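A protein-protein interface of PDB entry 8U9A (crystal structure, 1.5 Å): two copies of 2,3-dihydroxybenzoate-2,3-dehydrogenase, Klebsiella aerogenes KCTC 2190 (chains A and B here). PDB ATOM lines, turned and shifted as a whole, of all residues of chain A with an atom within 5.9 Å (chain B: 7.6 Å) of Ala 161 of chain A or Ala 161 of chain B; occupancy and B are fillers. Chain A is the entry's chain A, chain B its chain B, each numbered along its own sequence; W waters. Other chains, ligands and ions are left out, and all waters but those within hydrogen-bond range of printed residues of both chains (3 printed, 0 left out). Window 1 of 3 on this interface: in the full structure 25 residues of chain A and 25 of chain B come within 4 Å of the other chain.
Among the printed residues, merely in contact across the chains: Phe 111 of chain A with Phe 111 of chain B (3.9 Å), Phe 111 of chain A with Ala 161 of chain B (3.9 Å), Val 115 of chain A with Trp 107 of chain B (3.6 Å), Ala 157 of chain A with Ala 161 of chain B (3.3 Å), Ala 160 of chain A with Ala 160 of chain B (3.8 Å), Ala 160 of chain A with Ser 164 of chain B (3.8 Å), Ala 161 of chain A with Phe 111 of chain B (3.8 Å), Ala 161 of chain A with Ala 157 of chain B (3.3 Å), Ala 161 of chain A with Ala 161 of chain B (3.9 Å), Ser 164 of chain A with Gly 156 of chain B (3.5 Å) and Ser 164 of chain A with Ala 160 of chain B (3.8 Å).
The side-chain hydroxyl of Ser 164 of chain B is in hydrogen-bond range of the backbone NH of Ala 157 of chain A (3.3 Å).
The side-chain hydroxyl of Ser 164 of chain A is in hydrogen-bond range of the backbone NH of Ala 157 of chain B, 3.4 Å away.
The side-chain hydroxyl (OG) of Ser 164 of chain B sits close to the backbone carbonyl oxygen (O) of Gly 156 of chain A (3.5 Å).
Water W1 bridges the side-chain hydroxyl (OG) of Ser 164 of chain A (2.7 Å) and the backbone carbonyl oxygen (O) of Ala 145 of chain B (3.4 Å).
Water W2 lies within hydrogen-bond range of the side-chain hydroxyl (OG) of Ser 164 of chain A (2.8 Å), the backbone carbonyl oxygen (O) of Ser 153 of chain B (2.9 Å) and the backbone NH (N) of Ala 157 of chain B (3.5 Å).
Water W3 bridges the side-chain hydroxyl of Ser 164 of chain B (2.8 Å) and the backbone NH of Ala 157 of chain A (3.4 Å).
Phe 111 of chain A touches its own counterpart, Phe 111 of chain B.
Ala 157 of chain A touches Ser 164 of chain B, and with the chains exchanged Ser 164 of chain A touches Ala 157 of chain B.
Ala 160 of chain A touches its own counterpart, Ala 160 of chain B.
Ala 161 of chain A touches its own counterpart, Ala 161 of chain B.
13 positions are printed for both chains.
Of the 14 pairs that touch across the chains among the printed residues, 13 have their exchanged pair printed and touching as well.
The backbone carbonyl oxygen of Phe 111 of chain B is in hydrogen-bond range of the backbone NH of Gly 116 of chain B (3.0 Å).
Hydrophobic or aromatic side chains of chain B that line the printed part of chain A: Trp 107, Phe 111, Ala 157, Ala 160 and Ala 161.
Of the 13 printed residues of chain A, 7 touch a printed residue of chain B.
Printed residues of chain A that touch a printed residue of chain B: Phe 111, Val 115, Gly 156, Ala 157, Ala 160, Ala 161 and Ser 164.
Among the printed residues, 14 pairs touch across the chains.
Among the printed residues, no Asp or Glu carboxylate lies within 4 Å of a Lys or Arg side-chain nitrogen of the other chain.
Printed residues of chain B within 4 Å of Phe 111 of chain A: Phe 111 and Ala 161.
Of the printed residues of chain B, Val 115 of chain A touches Trp 107 (3.6 Å).
Ala 160 of chain A touches two residues of chain B.
Ala 161 of chain A touches three residues of chain B.
Lys 163 of chain A touches none of the printed residues of chain B.
Of the printed residues of chain A, Ala 161 of chain B touches Phe 111, Ala 157 and Ala 161.
The nearest residue of chain B that does not touch Ala 161 of chain A is Ala 160 of chain B (4.6 Å).
The nearest printed residue of chain B that does not touch Gly 156 of chain A is Ala 161 of chain B (6.0 Å).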
ATOM      1  N   PHE A 111      14.996 -20.167  14.490  1.00  0.00           N
ATOM      2  CA  PHE A 111      16.015 -19.135  14.666  1.00  0.00           C
ATOM      3  C   PHE A 111      15.665 -18.173  15.782  1.00  0.00           C
ATOM      4  O   PHE A 111      16.558 -17.790  16.548  1.00  0.00           O
ATOM      5  CB  PHE A 111      16.249 -18.400  13.343  1.00  0.00           C
ATOM      6  CG  PHE A 111      17.230 -19.127  12.482  1.00  0.00           C
ATOM      7  CD1 PHE A 111      16.809 -20.171  11.680  1.00  0.00           C
ATOM      8  CD2 PHE A 111      18.590 -18.832  12.553  1.00  0.00           C
ATOM      9  CE1 PHE A 111      17.713 -20.899  10.945  1.00  0.00           C
ATOM     10  CE2 PHE A 111      19.499 -19.558  11.821  1.00  0.00           C
ATOM     11  CZ  PHE A 111      19.064 -20.586  11.021  1.00  0.00           C
ATOM     12  N   VAL A 115      18.630 -18.906  18.387  1.00  0.00           N
ATOM     13  CA  VAL A 115      19.647 -17.862  18.300  1.00  0.00           C
ATOM     14  C   VAL A 115      19.164 -16.584  18.967  1.00  0.00           C
ATOM     15  O   VAL A 115      19.886 -15.963  19.745  1.00  0.00           O
ATOM     16  CB  VAL A 115      20.049 -17.568  16.835  1.00  0.00           C
ATOM     17  CG1 VAL A 115      21.373 -16.799  16.851  1.00  0.00           C
ATOM     18  CG2 VAL A 115      20.140 -18.828  15.993  1.00  0.00           C
ATOM     19  N   GLY A 156      20.573 -27.424  12.905  1.00  0.00           N
ATOM     20  CA  GLY A 156      22.025 -27.312  12.949  1.00  0.00           C
ATOM     21  C   GLY A 156      22.513 -25.927  12.592  1.00  0.00           C
ATOM     22  O   GLY A 156      23.458 -25.413  13.198  1.00  0.00           O
ATOM     23  N   ALA A 157      21.886 -25.302  11.607  1.00  0.00           N
ATOM     24  CA  ALA A 157      22.286 -23.960  11.231  1.00  0.00           C
ATOM     25  C   ALA A 157      22.037 -22.969  12.365  1.00  0.00           C
ATOM     26  O   ALA A 157      22.878 -22.105  12.630  1.00  0.00           O
ATOM     27  CB  ALA A 157      21.536 -23.560   9.962  1.00  0.00           C
ATOM     28  N   SER A 158      20.905 -23.089  13.056  1.00  0.00           N
ATOM     29  CA  SER A 158      20.620 -22.202  14.176  1.00  0.00           C
ATOM     30  C   SER A 158      21.617 -22.423  15.292  1.00  0.00           C
ATOM     31  O   SER A 158      22.059 -21.465  15.927  1.00  0.00           O
ATOM     32  CB  SER A 158      19.185 -22.412  14.651  1.00  0.00           C
ATOM     33  OG  SER A 158      19.004 -23.593  15.395  1.00  0.00           O
ATOM     34  N   LYS A 159      22.017 -23.664  15.503  1.00  0.00           N
ATOM     35  CA  LYS A 159      22.974 -23.946  16.568  1.00  0.00           C
ATOM     36  C   LYS A 159      24.371 -23.504  16.178  1.00  0.00           C
ATOM     37  O   LYS A 159      25.153 -23.095  17.041  1.00  0.00           O
ATOM     38  CB  LYS A 159      22.938 -25.426  16.924  1.00  0.00           C
ATOM     39  CG  LYS A 159      21.633 -25.847  17.619  1.00  0.00           C
ATOM     40  CD  LYS A 159      21.508 -25.225  18.988  1.00  0.00           C
ATOM     41  CE  LYS A 159      20.418 -25.907  19.829  1.00  0.00           C
ATOM     42  NZ  LYS A 159      20.498 -25.586  21.249  1.00  0.00           N
ATOM     43  N   ALA A 160      24.715 -23.554  14.882  1.00  0.00           N
ATOM     44  CA  ALA A 160      25.973 -22.980  14.424  1.00  0.00           C
ATOM     45  C   ALA A 160      25.998 -21.461  14.613  1.00  0.00           C
ATOM     46  O   ALA A 160      27.024 -20.897  15.005  1.00  0.00           O
ATOM     47  CB  ALA A 160      26.188 -23.353  12.957  1.00  0.00           C
ATOM     48  N   ALA A 161      24.872 -20.778  14.354  1.00  0.00           N
ATOM     49  CA  ALA A 161      24.818 -19.351  14.609  1.00  0.00           C
ATOM     50  C   ALA A 161      24.973 -19.079  16.089  1.00  0.00           C
ATOM     51  O   ALA A 161      25.699 -18.164  16.479  1.00  0.00           O
ATOM     52  CB  ALA A 161      23.498 -18.777  14.109  1.00  0.00           C
ATOM     53  N   LEU A 162      24.287 -19.870  16.920  1.00  0.00           N
ATOM     54  CA  LEU A 162      24.379 -19.705  18.371  1.00  0.00           C
ATOM     55  C   LEU A 162      25.818 -19.831  18.849  1.00  0.00           C
ATOM     56  O   LEU A 162      26.297 -19.003  19.642  1.00  0.00           O
ATOM     57  CB  LEU A 162      23.491 -20.734  19.072  1.00  0.00           C
ATOM     58  CG  LEU A 162      23.545 -20.726  20.592  1.00  0.00           C
ATOM     59  CD1 LEU A 162      23.036 -19.404  21.129  1.00  0.00           C
ATOM     60  CD2 LEU A 162      22.673 -21.821  21.083  1.00  0.00           C
ATOM     61  N   LYS A 163      26.511 -20.880  18.416  1.00  0.00           N
ATOM     62  CA  LYS A 163      27.910 -21.062  18.771  1.00  0.00           C
ATOM     63  C   LYS A 163      28.740 -19.859  18.354  1.00  0.00           C
ATOM     64  O   LYS A 163      29.544 -19.346  19.129  1.00  0.00           O
ATOM     65  CB  LYS A 163      28.452 -22.340  18.146  1.00  0.00           C
ATOM     66  CG  LYS A 163      29.923 -22.528  18.373  1.00  0.00           C
ATOM     67  CD  LYS A 163      30.385 -23.904  18.032  1.00  0.00           C
ATOM     68  CE  LYS A 163      31.881 -23.982  18.349  1.00  0.00           C
ATOM     69  NZ  LYS A 163      32.417 -25.334  18.122  1.00  0.00           N
ATOM     70  N   SER A 164      28.581 -19.400  17.114  1.00  0.00           N
ATOM     71  CA  SER A 164      29.370 -18.274  16.650  1.00  0.00           C
ATOM     72  C   SER A 164      29.119 -17.044  17.522  1.00  0.00           C
ATOM     73  O   SER A 164      30.050 -16.321  17.915  1.00  0.00           O
ATOM     74  CB  SER A 164      28.995 -17.997  15.201  1.00  0.00           C
ATOM     75  OG  SER A 164      29.656 -16.871  14.705  1.00  0.00           O
ATOM     76  N   LEU A 165      27.855 -16.766  17.775  1.00  0.00           N
ATOM     77  CA  LEU A 165      27.478 -15.628  18.595  1.00  0.00           C
ATOM     78  C   LEU A 165      28.098 -15.716  19.979  1.00  0.00           C
ATOM     79  O   LEU A 165      28.669 -14.737  20.474  1.00  0.00           O
ATOM     80  CB  LEU A 165      25.967 -15.571  18.689  1.00  0.00           C
ATOM     81  CG  LEU A 165      25.385 -14.497  19.616  1.00  0.00           C
ATOM     82  CD1 LEU A 165      25.594 -13.130  19.062  1.00  0.00           C
ATOM     83  CD2 LEU A 165      23.900 -14.774  19.864  1.00  0.00           C
ATOM     84  N   ALA A 166      27.975 -16.880  20.624  1.00  0.00           N
ATOM     85  CA  ALA A 166      28.526 -17.047  21.962  1.00  0.00           C
ATOM     86  C   ALA A 166      30.040 -16.842  21.975  1.00  0.00           C
ATOM     87  O   ALA A 166      30.573 -16.239  22.910  1.00  0.00           O
ATOM     88  CB  ALA A 166      28.154 -18.428  22.498  1.00  0.00           C
ATOM     89  N   TRP B 107      19.665  -6.978  13.532  1.00  0.00           N
ATOM     90  CA  TRP B 107      19.674  -8.415  13.817  1.00  0.00           C
ATOM     91  C   TRP B 107      18.747  -9.173  12.881  1.00  0.00           C
ATOM     92  O   TRP B 107      19.148 -10.160  12.250  1.00  0.00           O
ATOM     93  CB  TRP B 107      19.266  -8.640  15.278  1.00  0.00           C
ATOM     94  CG  TRP B 107      19.175 -10.072  15.656  1.00  0.00           C
ATOM     95  CD1 TRP B 107      18.042 -10.829  15.739  1.00  0.00           C
ATOM     96  CD2 TRP B 107      20.263 -10.936  15.991  1.00  0.00           C
ATOM     97  NE1 TRP B 107      18.355 -12.112  16.107  1.00  0.00           N
ATOM     98  CE2 TRP B 107      19.716 -12.202  16.273  1.00  0.00           C
ATOM     99  CE3 TRP B 107      21.650 -10.761  16.082  1.00  0.00           C
ATOM    100  CZ2 TRP B 107      20.502 -13.283  16.636  1.00  0.00           C
ATOM    101  CZ3 TRP B 107      22.423 -11.841  16.455  1.00  0.00           C
ATOM    102  CH2 TRP B 107      21.861 -13.075  16.725  1.00  0.00           C
ATOM    103  N   PHE B 111      19.806 -11.857   9.585  1.00  0.00           N
ATOM    104  CA  PHE B 111      19.493 -13.276   9.432  1.00  0.00           C
ATOM    105  C   PHE B 111      18.535 -13.506   8.277  1.00  0.00           C
ATOM    106  O   PHE B 111      18.700 -14.479   7.541  1.00  0.00           O
ATOM    107  CB  PHE B 111      18.960 -13.847  10.734  1.00  0.00           C
ATOM    108  CG  PHE B 111      20.056 -14.224  11.663  1.00  0.00           C
ATOM    109  CD1 PHE B 111      20.664 -13.277  12.464  1.00  0.00           C
ATOM    110  CD2 PHE B 111      20.513 -15.522  11.685  1.00  0.00           C
ATOM    111  CE1 PHE B 111      21.731 -13.623  13.271  1.00  0.00           C
ATOM    112  CE2 PHE B 111      21.560 -15.883  12.519  1.00  0.00           C
ATOM    113  CZ  PHE B 111      22.163 -14.917  13.305  1.00  0.00           C
ATOM    114  N   ASN B 114      20.958 -13.091   5.108  1.00  0.00           N
ATOM    115  CA  ASN B 114      22.177 -13.886   4.999  1.00  0.00           C
ATOM    116  C   ASN B 114      21.929 -15.375   5.158  1.00  0.00           C
ATOM    117  O   ASN B 114      22.708 -16.174   4.629  1.00  0.00           O
ATOM    118  CB  ASN B 114      23.216 -13.434   6.025  1.00  0.00           C
ATOM    119  CG  ASN B 114      23.737 -12.055   5.736  1.00  0.00           C
ATOM    120  OD1 ASN B 114      23.418 -11.464   4.708  1.00  0.00           O
ATOM    121  ND2 ASN B 114      24.546 -11.526   6.622  1.00  0.00           N
ATOM    122  N   VAL B 115      20.878 -15.784   5.840  1.00  0.00           N
ATOM    123  CA  VAL B 115      20.523 -17.192   5.980  1.00  0.00           C
ATOM    124  C   VAL B 115      19.212 -17.491   5.284  1.00  0.00           C
ATOM    125  O   VAL B 115      19.099 -18.465   4.545  1.00  0.00           O
ATOM    126  CB  VAL B 115      20.437 -17.624   7.466  1.00  0.00           C
ATOM    127  CG1 VAL B 115      20.525 -19.169   7.543  1.00  0.00           C
ATOM    128  CG2 VAL B 115      21.463 -16.922   8.339  1.00  0.00           C
ATOM    129  N   GLY B 116      18.190 -16.684   5.557  1.00  0.00           N
ATOM    130  CA  GLY B 116      16.890 -16.931   4.963  1.00  0.00           C
ATOM    131  C   GLY B 116      16.911 -16.899   3.448  1.00  0.00           C
ATOM    132  O   GLY B 116      16.161 -17.632   2.808  1.00  0.00           O
ATOM    133  N   ALA B 145      32.635 -16.268   9.687  1.00  0.00           N
ATOM    134  CA  ALA B 145      32.031 -17.521  10.114  1.00  0.00           C
ATOM    135  C   ALA B 145      33.029 -18.487  10.715  1.00  0.00           C
ATOM    136  O   ALA B 145      32.602 -19.475  11.322  1.00  0.00           O
ATOM    137  CB  ALA B 145      31.349 -18.198   8.940  1.00  0.00           C
ATOM    138  N   SER B 153      29.487  -9.833  15.530  1.00  0.00           N
ATOM    139  CA  SER B 153      28.914 -11.034  16.121  1.00  0.00           C
ATOM    140  C   SER B 153      27.709 -11.527  15.318  1.00  0.00           C
ATOM    141  O   SER B 153      27.607 -12.721  15.032  1.00  0.00           O
ATOM    142  CB  SER B 153      28.533 -10.793  17.587  1.00  0.00           C
ATOM    143  OG  SER B 153      27.503  -9.817  17.696  1.00  0.00           O
ATOM    144  N   ALA B 154      26.792 -10.627  14.938  1.00  0.00           N
ATOM    145  CA  ALA B 154      25.600 -11.066  14.219  1.00  0.00           C
ATOM    146  C   ALA B 154      25.937 -11.468  12.790  1.00  0.00           C
ATOM    147  O   ALA B 154      25.453 -12.489  12.295  1.00  0.00           O
ATOM    148  CB  ALA B 154      24.545  -9.961  14.211  1.00  0.00           C
ATOM    149  N   TYR B 155      26.752 -10.667  12.109  1.00  0.00           N
ATOM    150  CA  TYR B 155      27.163 -11.018  10.760  1.00  0.00           C
ATOM    151  C   TYR B 155      27.846 -12.374  10.733  1.00  0.00           C
ATOM    152  O   TYR B 155      27.498 -13.248   9.933  1.00  0.00           O
ATOM    153  CB  TYR B 155      28.102  -9.951  10.221  1.00  0.00           C
ATOM    154  CG  TYR B 155      28.596 -10.215   8.829  1.00  0.00           C
ATOM    155  CD1 TYR B 155      27.745 -10.097   7.739  1.00  0.00           C
ATOM    156  CD2 TYR B 155      29.910 -10.545   8.597  1.00  0.00           C
ATOM    157  CE1 TYR B 155      28.190 -10.306   6.451  1.00  0.00           C
ATOM    158  CE2 TYR B 155      30.375 -10.753   7.316  1.00  0.00           C
ATOM    159  CZ  TYR B 155      29.513 -10.634   6.250  1.00  0.00           C
ATOM    160  OH  TYR B 155      29.953 -10.830   4.970  1.00  0.00           O
ATOM    161  N   GLY B 156      28.841 -12.558  11.595  1.00  0.00           N
ATOM    162  CA  GLY B 156      29.516 -13.841  11.672  1.00  0.00           C
ATOM    163  C   GLY B 156      28.581 -14.995  11.972  1.00  0.00           C
ATOM    164  O   GLY B 156      28.712 -16.072  11.386  1.00  0.00           O
ATOM    165  N   ALA B 157      27.660 -14.795  12.912  1.00  0.00           N
ATOM    166  CA  ALA B 157      26.724 -15.844  13.285  1.00  0.00           C
ATOM    167  C   ALA B 157      25.805 -16.197  12.119  1.00  0.00           C
ATOM    168  O   ALA B 157      25.540 -17.380  11.868  1.00  0.00           O
ATOM    169  CB  ALA B 157      25.948 -15.401  14.529  1.00  0.00           C
ATOM    170  N   SER B 158      25.333 -15.188  11.383  1.00  0.00           N
ATOM    171  CA  SER B 158      24.491 -15.440  10.219  1.00  0.00           C
ATOM    172  C   SER B 158      25.255 -16.207   9.159  1.00  0.00           C
ATOM    173  O   SER B 158      24.693 -17.089   8.494  1.00  0.00           O
ATOM    174  CB  SER B 158      23.931 -14.121   9.697  1.00  0.00           C
ATOM    175  OG  SER B 158      24.874 -13.362   8.964  1.00  0.00           O
ATOM    176  N   LYS B 159      26.539 -15.893   8.981  1.00  0.00           N
ATOM    177  CA  LYS B 159      27.309 -16.606   7.979  1.00  0.00           C
ATOM    178  C   LYS B 159      27.670 -18.004   8.434  1.00  0.00           C
ATOM    179  O   LYS B 159      27.797 -18.905   7.608  1.00  0.00           O
ATOM    180  CB  LYS B 159      28.563 -15.795   7.630  1.00  0.00           C
ATOM    181  CG  LYS B 159      28.198 -14.487   6.916  1.00  0.00           C
ATOM    182  CD  LYS B 159      27.740 -14.784   5.475  1.00  0.00           C
ATOM    183  CE  LYS B 159      27.762 -13.546   4.574  1.00  0.00           C
ATOM    184  NZ  LYS B 159      27.551 -13.900   3.146  1.00  0.00           N
ATOM    185  N   ALA B 160      27.835 -18.215   9.738  1.00  0.00           N
ATOM    186  CA  ALA B 160      28.019 -19.561  10.255  1.00  0.00           C
ATOM    187  C   ALA B 160      26.761 -20.393  10.034  1.00  0.00           C
ATOM    188  O   ALA B 160      26.849 -21.576   9.703  1.00  0.00           O
ATOM    189  CB  ALA B 160      28.379 -19.509  11.741  1.00  0.00           C
ATOM    190  N   ALA B 161      25.588 -19.786  10.204  1.00  0.00           N
ATOM    191  CA  ALA B 161      24.350 -20.509   9.924  1.00  0.00           C
ATOM    192  C   ALA B 161      24.272 -20.842   8.448  1.00  0.00           C
ATOM    193  O   ALA B 161      23.939 -21.963   8.076  1.00  0.00           O
ATOM    194  CB  ALA B 161      23.133 -19.684  10.343  1.00  0.00           C
ATOM    195  N   LEU B 162      24.591 -19.869   7.599  1.00  0.00           N
ATOM    196  CA  LEU B 162      24.564 -20.098   6.161  1.00  0.00           C
ATOM    197  C   LEU B 162      25.484 -21.251   5.783  1.00  0.00           C
ATOM    198  O   LEU B 162      25.115 -22.123   4.980  1.00  0.00           O
ATOM    199  CB  LEU B 162      24.966 -18.807   5.460  1.00  0.00           C
ATOM    200  CG  LEU B 162      25.097 -18.900   3.929  1.00  0.00           C
ATOM    201  CD1 LEU B 162      23.791 -19.278   3.307  1.00  0.00           C
ATOM    202  CD2 LEU B 162      25.610 -17.581   3.406  1.00  0.00           C
ATOM    203  N   LYS B 163      26.702 -21.260   6.315  1.00  0.00           N
ATOM    204  CA  LYS B 163      27.623 -22.344   5.989  1.00  0.00           C
ATOM    205  C   LYS B 163      27.035 -23.687   6.405  1.00  0.00           C
ATOM    206  O   LYS B 163      27.059 -24.657   5.645  1.00  0.00           O
ATOM    207  CB  LYS B 163      28.977 -22.102   6.655  1.00  0.00           C
ATOM    208  CG  LYS B 163      29.905 -23.262   6.535  1.00  0.00           C
ATOM    209  CD  LYS B 163      31.313 -22.921   6.951  1.00  0.00           C
ATOM    210  CE  LYS B 163      32.178 -24.176   6.799  1.00  0.00           C
ATOM    211  NZ  LYS B 163      33.586 -23.889   7.038  1.00  0.00           N
ATOM    212  N   SER B 164      26.509 -23.768   7.628  1.00  0.00           N
ATOM    213  CA  SER B 164      25.935 -25.017   8.108  1.00  0.00           C
ATOM    214  C   SER B 164      24.791 -25.471   7.216  1.00  0.00           C
ATOM    215  O   SER B 164      24.689 -26.652   6.857  1.00  0.00           O
ATOM    216  CB  SER B 164      25.465 -24.816   9.545  1.00  0.00           C
ATOM    217  OG  SER B 164      24.783 -25.925  10.052  1.00  0.00           O
ATOM    218  N   LEU B 165      23.894 -24.550   6.885  1.00  0.00           N
ATOM    219  CA  LEU B 165      22.778 -24.859   5.998  1.00  0.00           C
ATOM    220  C   LEU B 165      23.268 -25.384   4.660  1.00  0.00           C
ATOM    221  O   LEU B 165      22.798 -26.419   4.171  1.00  0.00           O
ATOM    222  CB  LEU B 165      21.937 -23.602   5.806  1.00  0.00           C
ATOM    223  CG  LEU B 165      20.831 -23.727   4.771  1.00  0.00           C
ATOM    224  CD1 LEU B 165      19.761 -24.665   5.250  1.00  0.00           C
ATOM    225  CD2 LEU B 165      20.244 -22.346   4.463  1.00  0.00           C
ATOM    226  N   ALA B 166      24.213 -24.679   4.051  1.00  0.00           N
ATOM    227  CA  ALA B 166      24.714 -25.098   2.746  1.00  0.00           C
ATOM    228  C   ALA B 166      25.337 -26.491   2.798  1.00  0.00           C
ATOM    229  O   ALA B 166      25.174 -27.279   1.855  1.00  0.00           O
ATOM    230  CB  ALA B 166      25.704 -24.055   2.231  1.00  0.00           C
ATOM    231  N   LEU B 167      26.070 -26.819   3.874  1.00  0.00           N
ATOM    232  CA  LEU B 167      26.675 -28.139   3.971  1.00  0.00           C
ATOM    233  C   LEU B 167      25.610 -29.213   4.142  1.00  0.00           C
ATOM    234  O   LEU B 167      25.744 -30.302   3.593  1.00  0.00           O
ATOM    235  CB  LEU B 167      27.702 -28.195   5.110  1.00  0.00           C
ATOM    236  CG  LEU B 167      28.918 -27.266   4.916  1.00  0.00           C
ATOM    237  CD1 LEU B 167      29.820 -27.282   6.174  1.00  0.00           C
ATOM    238  CD2 LEU B 167      29.703 -27.628   3.702  1.00  0.00           C
ATOM    239  N   LEU B 182      31.546 -23.794  -0.667  1.00  0.00           N
ATOM    240  CA  LEU B 182      31.492 -22.413  -0.235  1.00  0.00           C
ATOM    241  C   LEU B 182      32.818 -21.722  -0.482  1.00  0.00           C
ATOM    242  O   LEU B 182      33.869 -22.354  -0.566  1.00  0.00           O
ATOM    243  CB  LEU B 182      31.186 -22.300   1.263  1.00  0.00           C
ATOM    244  CG  LEU B 182      29.809 -22.829   1.673  1.00  0.00           C
ATOM    245  CD1 LEU B 182      30.028 -24.167   2.366  1.00  0.00           C
ATOM    246  CD2 LEU B 182      29.081 -21.859   2.579  1.00  0.00           C
HETATM  247  O   HOH W   1      32.124 -17.162  13.736  1.00  0.00           O
HETATM  248  O   HOH W   2      30.027 -14.198  15.368  1.00  0.00           O
HETATM  249  O   HOH W   3      22.768 -27.711   9.319  1.00  0.00           O
